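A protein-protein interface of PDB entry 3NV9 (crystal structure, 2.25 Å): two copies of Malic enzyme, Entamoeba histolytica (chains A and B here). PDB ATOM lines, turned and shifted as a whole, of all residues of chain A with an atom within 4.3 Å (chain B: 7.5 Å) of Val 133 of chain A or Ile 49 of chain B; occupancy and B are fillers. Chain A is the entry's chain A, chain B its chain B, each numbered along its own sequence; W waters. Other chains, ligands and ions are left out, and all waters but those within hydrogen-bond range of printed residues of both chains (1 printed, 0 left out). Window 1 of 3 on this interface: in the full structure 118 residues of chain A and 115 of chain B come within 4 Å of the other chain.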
ATOM      1  N   ILE A  47      25.396 -16.907   0.036  1.00  0.00           N
ATOM      2  CA  ILE A  47      24.400 -17.643  -0.770  1.00  0.00           C
ATOM      3  C   ILE A  47      23.682 -16.749  -1.805  1.00  0.00           C
ATOM      4  O   ILE A  47      23.685 -15.529  -1.701  1.00  0.00           O
ATOM      5  CB  ILE A  47      23.361 -18.438   0.090  1.00  0.00           C
ATOM      6  CG1 ILE A  47      22.431 -17.466   0.807  1.00  0.00           C
ATOM      7  CG2 ILE A  47      24.057 -19.262   1.138  1.00  0.00           C
ATOM      8  CD1 ILE A  47      21.274 -18.171   1.620  1.00  0.00           C
ATOM      9  N   GLN A  48      23.068 -17.373  -2.800  1.00  0.00           N
ATOM     10  CA  GLN A  48      22.383 -16.668  -3.836  1.00  0.00           C
ATOM     11  C   GLN A  48      21.208 -17.500  -4.305  1.00  0.00           C
ATOM     12  O   GLN A  48      21.060 -18.650  -3.967  1.00  0.00           O
ATOM     13  CB  GLN A  48      23.341 -16.385  -4.985  1.00  0.00           C
ATOM     14  CG  GLN A  48      23.939 -17.656  -5.612  1.00  0.00           C
ATOM     15  CD  GLN A  48      24.658 -17.407  -6.949  1.00  0.00           C
ATOM     16  OE1 GLN A  48      24.354 -16.464  -7.697  1.00  0.00           O
ATOM     17  NE2 GLN A  48      25.663 -18.231  -7.211  1.00  0.00           N
ATOM     18  N   ILE A  49      20.344 -16.905  -5.095  1.00  0.00           N
ATOM     19  CA  ILE A  49      19.272 -17.662  -5.677  1.00  0.00           C
ATOM     20  C   ILE A  49      19.696 -18.070  -7.087  1.00  0.00           C
ATOM     21  O   ILE A  49      20.483 -17.402  -7.712  1.00  0.00           O
ATOM     22  CB  ILE A  49      17.961 -16.842  -5.646  1.00  0.00           C
ATOM     23  CG1 ILE A  49      17.199 -17.079  -4.338  1.00  0.00           C
ATOM     24  CG2 ILE A  49      17.020 -17.293  -6.752  1.00  0.00           C
ATOM     25  CD1 ILE A  49      17.913 -16.691  -3.090  1.00  0.00           C
ATOM     26  N   PHE A  92      12.200 -26.390   1.022  1.00  0.00           N
ATOM     27  CA  PHE A  92      12.532 -24.978   1.424  1.00  0.00           C
ATOM     28  C   PHE A  92      12.483 -24.853   2.935  1.00  0.00           C
ATOM     29  O   PHE A  92      11.423 -25.116   3.566  1.00  0.00           O
ATOM     30  CB  PHE A  92      11.550 -23.959   0.766  1.00  0.00           C
ATOM     31  CG  PHE A  92      12.057 -22.515   0.670  1.00  0.00           C
ATOM     32  CD1 PHE A  92      13.442 -22.213   0.590  1.00  0.00           C
ATOM     33  CD2 PHE A  92      11.140 -21.460   0.551  1.00  0.00           C
ATOM     34  CE1 PHE A  92      13.899 -20.867   0.444  1.00  0.00           C
ATOM     35  CE2 PHE A  92      11.566 -20.111   0.411  1.00  0.00           C
ATOM     36  CZ  PHE A  92      12.955 -19.809   0.371  1.00  0.00           C
ATOM     37  N   VAL A  93      13.614 -24.451   3.520  1.00  0.00           N
ATOM     38  CA  VAL A  93      13.749 -24.325   4.951  1.00  0.00           C
ATOM     39  C   VAL A  93      13.975 -22.870   5.327  1.00  0.00           C
ATOM     40  O   VAL A  93      14.772 -22.204   4.657  1.00  0.00           O
ATOM     41  CB  VAL A  93      14.850 -25.221   5.503  1.00  0.00           C
ATOM     42  CG1 VAL A  93      15.126 -24.891   6.971  1.00  0.00           C
ATOM     43  CG2 VAL A  93      14.408 -26.747   5.346  1.00  0.00           C
ATOM     44  N   GLY A  94      13.228 -22.361   6.329  1.00  0.00           N
ATOM     45  CA  GLY A  94      13.466 -21.006   6.856  1.00  0.00           C
ATOM     46  C   GLY A  94      14.308 -21.034   8.117  1.00  0.00           C
ATOM     47  O   GLY A  94      13.992 -21.758   9.031  1.00  0.00           O
ATOM     48  N   VAL A  95      15.408 -20.306   8.136  1.00  0.00           N
ATOM     49  CA  VAL A  95      16.292 -20.299   9.293  1.00  0.00           C
ATOM     50  C   VAL A  95      15.841 -19.055  10.035  1.00  0.00           C
ATOM     51  O   VAL A  95      16.231 -17.946   9.664  1.00  0.00           O
ATOM     52  CB  VAL A  95      17.816 -20.183   8.863  1.00  0.00           C
ATOM     53  CG1 VAL A  95      18.808 -20.328  10.029  1.00  0.00           C
ATOM     54  CG2 VAL A  95      18.173 -21.301   7.837  1.00  0.00           C
ATOM     55  N   ALA A 121      22.325 -21.540   6.235  1.00  0.00           N
ATOM     56  CA  ALA A 121      21.631 -21.813   5.002  1.00  0.00           C
ATOM     57  C   ALA A 121      22.648 -22.366   4.018  1.00  0.00           C
ATOM     58  O   ALA A 121      22.290 -23.247   3.254  1.00  0.00           O
ATOM     59  CB  ALA A 121      21.030 -20.559   4.438  1.00  0.00           C
ATOM     60  N   LYS A 125      22.520 -26.306   2.161  1.00  0.00           N
ATOM     61  CA  LYS A 125      22.593 -26.613   0.746  1.00  0.00           C
ATOM     62  C   LYS A 125      23.749 -27.564   0.469  1.00  0.00           C
ATOM     63  O   LYS A 125      23.542 -28.591  -0.142  1.00  0.00           O
ATOM     64  CB  LYS A 125      22.722 -25.357  -0.106  1.00  0.00           C
ATOM     65  CG  LYS A 125      22.767 -25.695  -1.598  1.00  0.00           C
ATOM     66  CD  LYS A 125      21.434 -26.180  -2.117  1.00  0.00           C
ATOM     67  CE  LYS A 125      21.451 -26.203  -3.630  1.00  0.00           C
ATOM     68  NZ  LYS A 125      20.085 -26.427  -4.147  1.00  0.00           N
ATOM     69  N   ASP A 131      17.239 -26.390   0.209  1.00  0.00           N
ATOM     70  CA  ASP A 131      17.212 -24.912  -0.112  1.00  0.00           C
ATOM     71  C   ASP A 131      16.781 -24.120   1.126  1.00  0.00           C
ATOM     72  O   ASP A 131      15.783 -24.423   1.711  1.00  0.00           O
ATOM     73  CB  ASP A 131      16.323 -24.626  -1.309  1.00  0.00           C
ATOM     74  CG  ASP A 131      16.869 -25.284  -2.576  1.00  0.00           C
ATOM     75  OD1 ASP A 131      18.000 -24.954  -2.983  1.00  0.00           O
ATOM     76  OD2 ASP A 131      16.179 -26.143  -3.156  1.00  0.00           O
ATOM     77  N   ALA A 132      17.553 -23.149   1.576  1.00  0.00           N
ATOM     78  CA  ALA A 132      17.250 -22.511   2.860  1.00  0.00           C
ATOM     79  C   ALA A 132      17.683 -21.047   2.794  1.00  0.00           C
ATOM     80  O   ALA A 132      18.617 -20.712   2.063  1.00  0.00           O
ATOM     81  CB  ALA A 132      17.923 -23.210   3.938  1.00  0.00           C
ATOM     82  N   VAL A 133      16.950 -20.165   3.476  1.00  0.00           N
ATOM     83  CA  VAL A 133      17.353 -18.802   3.530  1.00  0.00           C
ATOM     84  C   VAL A 133      17.306 -18.252   4.971  1.00  0.00           C
ATOM     85  O   VAL A 133      16.509 -18.672   5.779  1.00  0.00           O
ATOM     86  CB  VAL A 133      16.575 -17.891   2.560  1.00  0.00           C
ATOM     87  CG1 VAL A 133      17.003 -18.151   1.119  1.00  0.00           C
ATOM     88  CG2 VAL A 133      15.102 -17.962   2.774  1.00  0.00           C
ATOM     89  N   PRO A 134      18.205 -17.319   5.288  1.00  0.00           N
ATOM     90  CA  PRO A 134      18.078 -16.696   6.614  1.00  0.00           C
ATOM     91  C   PRO A 134      16.734 -15.917   6.723  1.00  0.00           C
ATOM     92  O   PRO A 134      16.295 -15.265   5.735  1.00  0.00           O
ATOM     93  CB  PRO A 134      19.300 -15.773   6.682  1.00  0.00           C
ATOM     94  CG  PRO A 134      19.782 -15.609   5.236  1.00  0.00           C
ATOM     95  CD  PRO A 134      19.145 -16.630   4.386  1.00  0.00           C
ATOM     96  N   ILE A 135      16.048 -16.023   7.878  1.00  0.00           N
ATOM     97  CA  ILE A 135      14.890 -15.151   8.168  1.00  0.00           C
ATOM     98  C   ILE A 135      15.119 -14.517   9.506  1.00  0.00           C
ATOM     99  O   ILE A 135      14.721 -15.063  10.504  1.00  0.00           O
ATOM    100  CB  ILE A 135      13.580 -15.938   8.216  1.00  0.00           C
ATOM    101  CG1 ILE A 135      13.354 -16.698   6.904  1.00  0.00           C
ATOM    102  CG2 ILE A 135      12.342 -15.027   8.517  1.00  0.00           C
ATOM    103  CD1 ILE A 135      12.862 -15.829   5.749  1.00  0.00           C
ATOM    104  N   ILE B  47      13.086 -22.031  -8.596  1.00  0.00           N
ATOM    105  CA  ILE B  47      14.364 -21.523  -8.065  1.00  0.00           C
ATOM    106  C   ILE B  47      15.038 -22.432  -7.005  1.00  0.00           C
ATOM    107  O   ILE B  47      14.453 -23.371  -6.531  1.00  0.00           O
ATOM    108  CB  ILE B  47      14.232 -20.111  -7.488  1.00  0.00           C
ATOM    109  CG1 ILE B  47      13.470 -20.107  -6.120  1.00  0.00           C
ATOM    110  CG2 ILE B  47      13.724 -19.220  -8.525  1.00  0.00           C
ATOM    111  CD1 ILE B  47      13.172 -18.653  -5.545  1.00  0.00           C
ATOM    112  N   GLN B  48      16.265 -22.118  -6.623  1.00  0.00           N
ATOM    113  CA  GLN B  48      16.983 -22.932  -5.617  1.00  0.00           C
ATOM    114  C   GLN B  48      18.002 -21.991  -5.011  1.00  0.00           C
ATOM    115  O   GLN B  48      18.267 -20.943  -5.576  1.00  0.00           O
ATOM    116  CB  GLN B  48      17.715 -24.112  -6.302  1.00  0.00           C
ATOM    117  CG  GLN B  48      18.988 -23.733  -7.109  1.00  0.00           C
ATOM    118  CD  GLN B  48      19.694 -24.967  -7.692  1.00  0.00           C
ATOM    119  OE1 GLN B  48      19.723 -26.016  -7.066  1.00  0.00           O
ATOM    120  NE2 GLN B  48      20.205 -24.858  -8.895  1.00  0.00           N
ATOM    121  N   ILE B  49      18.547 -22.331  -3.863  1.00  0.00           N
ATOM    122  CA  ILE B  49      19.597 -21.519  -3.292  1.00  0.00           C
ATOM    123  C   ILE B  49      20.959 -22.138  -3.687  1.00  0.00           C
ATOM    124  O   ILE B  49      21.079 -23.363  -3.745  1.00  0.00           O
ATOM    125  CB  ILE B  49      19.471 -21.508  -1.768  1.00  0.00           C
ATOM    126  CG1 ILE B  49      18.573 -20.365  -1.306  1.00  0.00           C
ATOM    127  CG2 ILE B  49      20.798 -21.202  -1.186  1.00  0.00           C
ATOM    128  CD1 ILE B  49      17.148 -20.566  -1.568  1.00  0.00           C
ATOM    129  N   MET B  50      21.985 -21.315  -3.907  1.00  0.00           N
ATOM    130  CA  MET B  50      23.333 -21.834  -4.224  1.00  0.00           C
ATOM    131  C   MET B  50      24.428 -21.090  -3.447  1.00  0.00           C
ATOM    132  O   MET B  50      24.268 -19.904  -3.216  1.00  0.00           O
ATOM    133  CB  MET B  50      23.553 -21.625  -5.736  1.00  0.00           C
ATOM    134  CG  MET B  50      24.705 -22.376  -6.300  1.00  0.00           C
ATOM    135  SD  MET B  50      24.463 -24.192  -6.378  1.00  0.00           S
ATOM    136  CE  MET B  50      23.126 -24.072  -7.579  1.00  0.00           C
ATOM    137  N   PRO B  51      25.585 -21.739  -3.134  1.00  0.00           N
ATOM    138  CA  PRO B  51      26.729 -20.919  -2.662  1.00  0.00           C
ATOM    139  C   PRO B  51      27.087 -19.850  -3.683  1.00  0.00           C
ATOM    140  O   PRO B  51      26.795 -20.040  -4.863  1.00  0.00           O
ATOM    141  CB  PRO B  51      27.909 -21.927  -2.566  1.00  0.00           C
ATOM    142  CG  PRO B  51      27.183 -23.299  -2.285  1.00  0.00           C
ATOM    143  CD  PRO B  51      25.937 -23.190  -3.239  1.00  0.00           C
ATOM    144  N   LEU B  88      23.843 -11.404   2.221  1.00  0.00           N
ATOM    145  CA  LEU B  88      23.204 -11.268   0.918  1.00  0.00           C
ATOM    146  C   LEU B  88      22.185 -10.117   0.940  1.00  0.00           C
ATOM    147  O   LEU B  88      21.638  -9.739  -0.097  1.00  0.00           O
ATOM    148  CB  LEU B  88      22.536 -12.589   0.532  1.00  0.00           C
ATOM    149  CG  LEU B  88      21.158 -12.875   1.181  1.00  0.00           C
ATOM    150  CD1 LEU B  88      20.481 -14.047   0.507  1.00  0.00           C
ATOM    151  CD2 LEU B  88      21.240 -13.115   2.706  1.00  0.00           C
ATOM    152  N   PHE B  92      18.965  -8.712  -1.778  1.00  0.00           N
ATOM    153  CA  PHE B  92      17.944  -9.699  -1.387  1.00  0.00           C
ATOM    154  C   PHE B  92      16.617  -8.965  -1.264  1.00  0.00           C
ATOM    155  O   PHE B  92      16.467  -8.043  -0.445  1.00  0.00           O
ATOM    156  CB  PHE B  92      18.325 -10.294  -0.045  1.00  0.00           C
ATOM    157  CG  PHE B  92      17.715 -11.632   0.261  1.00  0.00           C
ATOM    158  CD1 PHE B  92      17.367 -12.537  -0.740  1.00  0.00           C
ATOM    159  CD2 PHE B  92      17.549 -12.017   1.579  1.00  0.00           C
ATOM    160  CE1 PHE B  92      16.825 -13.787  -0.412  1.00  0.00           C
ATOM    161  CE2 PHE B  92      16.993 -13.285   1.928  1.00  0.00           C
ATOM    162  CZ  PHE B  92      16.632 -14.164   0.919  1.00  0.00           C
ATOM    163  N   ALA B 132      16.084 -13.217  -4.743  1.00  0.00           N
ATOM    164  CA  ALA B 132      14.760 -13.015  -4.221  1.00  0.00           C
ATOM    165  C   ALA B 132      14.106 -14.336  -3.935  1.00  0.00           C
ATOM    166  O   ALA B 132      14.288 -15.307  -4.674  1.00  0.00           O
ATOM    167  CB  ALA B 132      13.914 -12.262  -5.224  1.00  0.00           C
ATOM    168  N   VAL B 133      13.277 -14.341  -2.890  1.00  0.00           N
ATOM    169  CA  VAL B 133      12.426 -15.475  -2.589  1.00  0.00           C
ATOM    170  C   VAL B 133      10.940 -15.084  -2.385  1.00  0.00           C
ATOM    171  O   VAL B 133      10.625 -13.911  -2.095  1.00  0.00           O
ATOM    172  CB  VAL B 133      12.975 -16.237  -1.376  1.00  0.00           C
ATOM    173  CG1 VAL B 133      14.334 -16.898  -1.719  1.00  0.00           C
ATOM    174  CG2 VAL B 133      13.093 -15.316  -0.164  1.00  0.00           C
ATOM    175  N   PRO B 134      10.018 -16.067  -2.588  1.00  0.00           N
ATOM    176  CA  PRO B 134       8.607 -15.884  -2.320  1.00  0.00           C
ATOM    177  C   PRO B 134       8.372 -15.921  -0.803  1.00  0.00           C
ATOM    178  O   PRO B 134       9.011 -16.701  -0.107  1.00  0.00           O
ATOM    179  CB  PRO B 134       7.959 -17.132  -2.974  1.00  0.00           C
ATOM    180  CG  PRO B 134       9.053 -18.121  -3.072  1.00  0.00           C
ATOM    181  CD  PRO B 134      10.282 -17.342  -3.289  1.00  0.00           C
ATOM    182  N   ILE B 135       7.474 -15.072  -0.312  1.00  0.00           N
ATOM    183  CA  ILE B 135       7.171 -14.974   1.106  1.00  0.00           C
ATOM    184  C   ILE B 135       5.647 -14.828   1.074  1.00  0.00           C
ATOM    185  O   ILE B 135       5.119 -13.725   0.985  1.00  0.00           O
ATOM    186  CB  ILE B 135       7.819 -13.728   1.791  1.00  0.00           C
ATOM    187  CG1 ILE B 135       9.370 -13.723   1.701  1.00  0.00           C
ATOM    188  CG2 ILE B 135       7.240 -13.519   3.243  1.00  0.00           C
ATOM    189  CD1 ILE B 135      10.100 -14.891   2.327  1.00  0.00           C
ATOM    190  N   THR B 161      16.011  -8.747   7.194  1.00  0.00           N
ATOM    191  CA  THR B 161      16.564  -9.765   6.354  1.00  0.00           C
ATOM    192  C   THR B 161      16.825  -9.248   4.972  1.00  0.00           C
ATOM    193  O   THR B 161      17.689  -9.783   4.274  1.00  0.00           O
ATOM    194  CB  THR B 161      15.580 -10.918   6.256  1.00  0.00           C
ATOM    195  OG1 THR B 161      15.430 -11.516   7.559  1.00  0.00           O
ATOM    196  CG2 THR B 161      16.102 -11.995   5.276  1.00  0.00           C
ATOM    197  N   PHE B 162      16.109  -8.187   4.568  1.00  0.00           N
ATOM    198  CA  PHE B 162      16.018  -7.841   3.151  1.00  0.00           C
ATOM    199  C   PHE B 162      16.627  -6.517   2.744  1.00  0.00           C
ATOM    200  O   PHE B 162      16.935  -5.653   3.585  1.00  0.00           O
ATOM    201  CB  PHE B 162      14.553  -7.932   2.674  1.00  0.00           C
ATOM    202  CG  PHE B 162      14.030  -9.372   2.584  1.00  0.00           C
ATOM    203  CD1 PHE B 162      14.518 -10.243   1.593  1.00  0.00           C
ATOM    204  CD2 PHE B 162      13.054  -9.848   3.465  1.00  0.00           C
ATOM    205  CE1 PHE B 162      14.063 -11.575   1.510  1.00  0.00           C
ATOM    206  CE2 PHE B 162      12.590 -11.169   3.392  1.00  0.00           C
ATOM    207  CZ  PHE B 162      13.096 -12.044   2.396  1.00  0.00           C
HETATM  208  O   HOH W   1      13.920 -25.537  -4.540  1.00  0.00           O
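Ile 47 of chain A touches Ile 49 of chain B. Gln 48 of chain A touches Gln 48 of chain B (O to O, 3.96 Å). Ile 49 of chain A touches Ala 132 of chain B (CG1 to O, 3.4 Å). Ile 49 of chain A touches Val 133 of chain B. Ile 49 of chain B touches Phe 92 of chain A. CZ of Phe 92 of chain A touches CG1 of Val 133 of chain B, at 3.8 Å. Asp 131 of chain A touches Gln 48 of chain B. Ile 49 of chain B touches Val 133 of chain A. O of Pro 134 of chain A touches CG2 of Thr 161 of chain B (3.3 Å). Thr 161 of chain B touches Ile 135 of chain A (OG1 to C, 3.6 Å).
Printed residues of chain B that touch a printed residue of chain A: Gln 48, Ile 49, Met 50, Pro 51, Leu 88, Ala 132, Val 133 and Thr 161. Hydrophobic or aromatic side chains of chain B within 4 Å of the printed part of chain A: Ile 49, Met 50, Leu 88 and Val 133. Among the printed residues, 21 pairs touch across the chains. Among the printed residues, no Asp or Glu carboxylate lies within 4 Å of a Lys or Arg side-chain nitrogen of the other chain.
Of the printed residues of chain B, Val 133 of chain A touches Ile 49 (3.6 Å). Ile 49 of chain B touches just these residues of chain A: Ile 47 (3.98 Å), Gln 48 (3.3 Å), Phe 92 (3.8 Å), Lys 125 (2.9 Å), Asp 131 (2.8 Å), Ala 132 (3.4 Å) and Val 133 (3.6 Å). Of the printed residues of chain A, Leu 88 of chain B touches Ile 47 (3.9 Å) and Pro 134 (3.8 Å). Printed residues of chain A within 4 Å of Val 133 of chain B: Ile 49 and Phe 92. The nearest printed residue of chain B that does not touch Val 133 of chain A is Phe 92 of chain B (4.01 Å). The nearest residue of chain A that does not touch Ile 49 of chain B is Ile 49 of chain A (4.1 Å).
Water W1 lies within hydrogen-bond range of the side-chain carboxylate (OD2) of Asp 131 of chain A (2.7 Å) and the backbone carbonyl oxygen (O) of Ile 47 of chain B (3.0 Å).
The backbone carbonyl oxygen (O) of Gln 48 of chain A sits at hydrogen-bond distance from the backbone NH (N) of Met 50 of chain B (2.8 Å). O of Ile 49 of chain B lies close to NZ of Lys 125 of chain A, at 3.2 Å. The side-chain amino group (NZ) of Lys 125 of chain A lies within hydrogen-bond range of the side-chain amide oxygen (OE1) of Gln 48 of chain B (3.0 Å). NE2 of Gln 48 of chain A is in hydrogen-bond range of O of Pro 51 of chain B (3.2 Å). OD1 of Asp 131 of chain A is in hydrogen-bond range of N of Ile 49 of chain B.
Gln 48 of chain B touches its own counterpart, Gln 48 of chain A. Ile 49 of chain A touches Val 133 of chain B, and with the chains exchanged Val 133 of chain A touches Ile 49 of chain B. Phe 92 of chain A touches Ile 49 of chain B, but with the chains exchanged Ile 49 of chain A does not touch Phe 92 of chain B (4.1 Å). Phe 92 of chain A touches Val 133 of chain B, but with the chains exchanged Val 133 of chain A does not touch Phe 92 of chain B (4.01 Å). Positions printed for both chains: 47, 48, 49, 92, 132, 133, 134 and 135. Of the 21 pairs that touch across the chains among the printed residues, 7 have their exchanged pair printed and touching as well.
The backbone carbonyl oxygen of Asp 131 of chain A sits at hydrogen-bond distance from the backbone NH of Val 93 of chain A. The backbone carbonyl oxygen of Val 93 of chain A sits at hydrogen-bond distance from the backbone NH of Val 133 of chain A (3.2 Å). O of Val 133 of chain A is in hydrogen-bond range of N of Val 95 of chain A. The side-chain carboxylate (OD1) of Asp 131 of chain A lies within salt-bridge range of the side-chain amino group (NZ) of Lys 125 of chain A (2.8 Å). The backbone carbonyl oxygen (O) of Val 95 of chain A lies within hydrogen-bond range of the backbone NH (N) of Ile 135 of chain A, 2.6 Å away.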
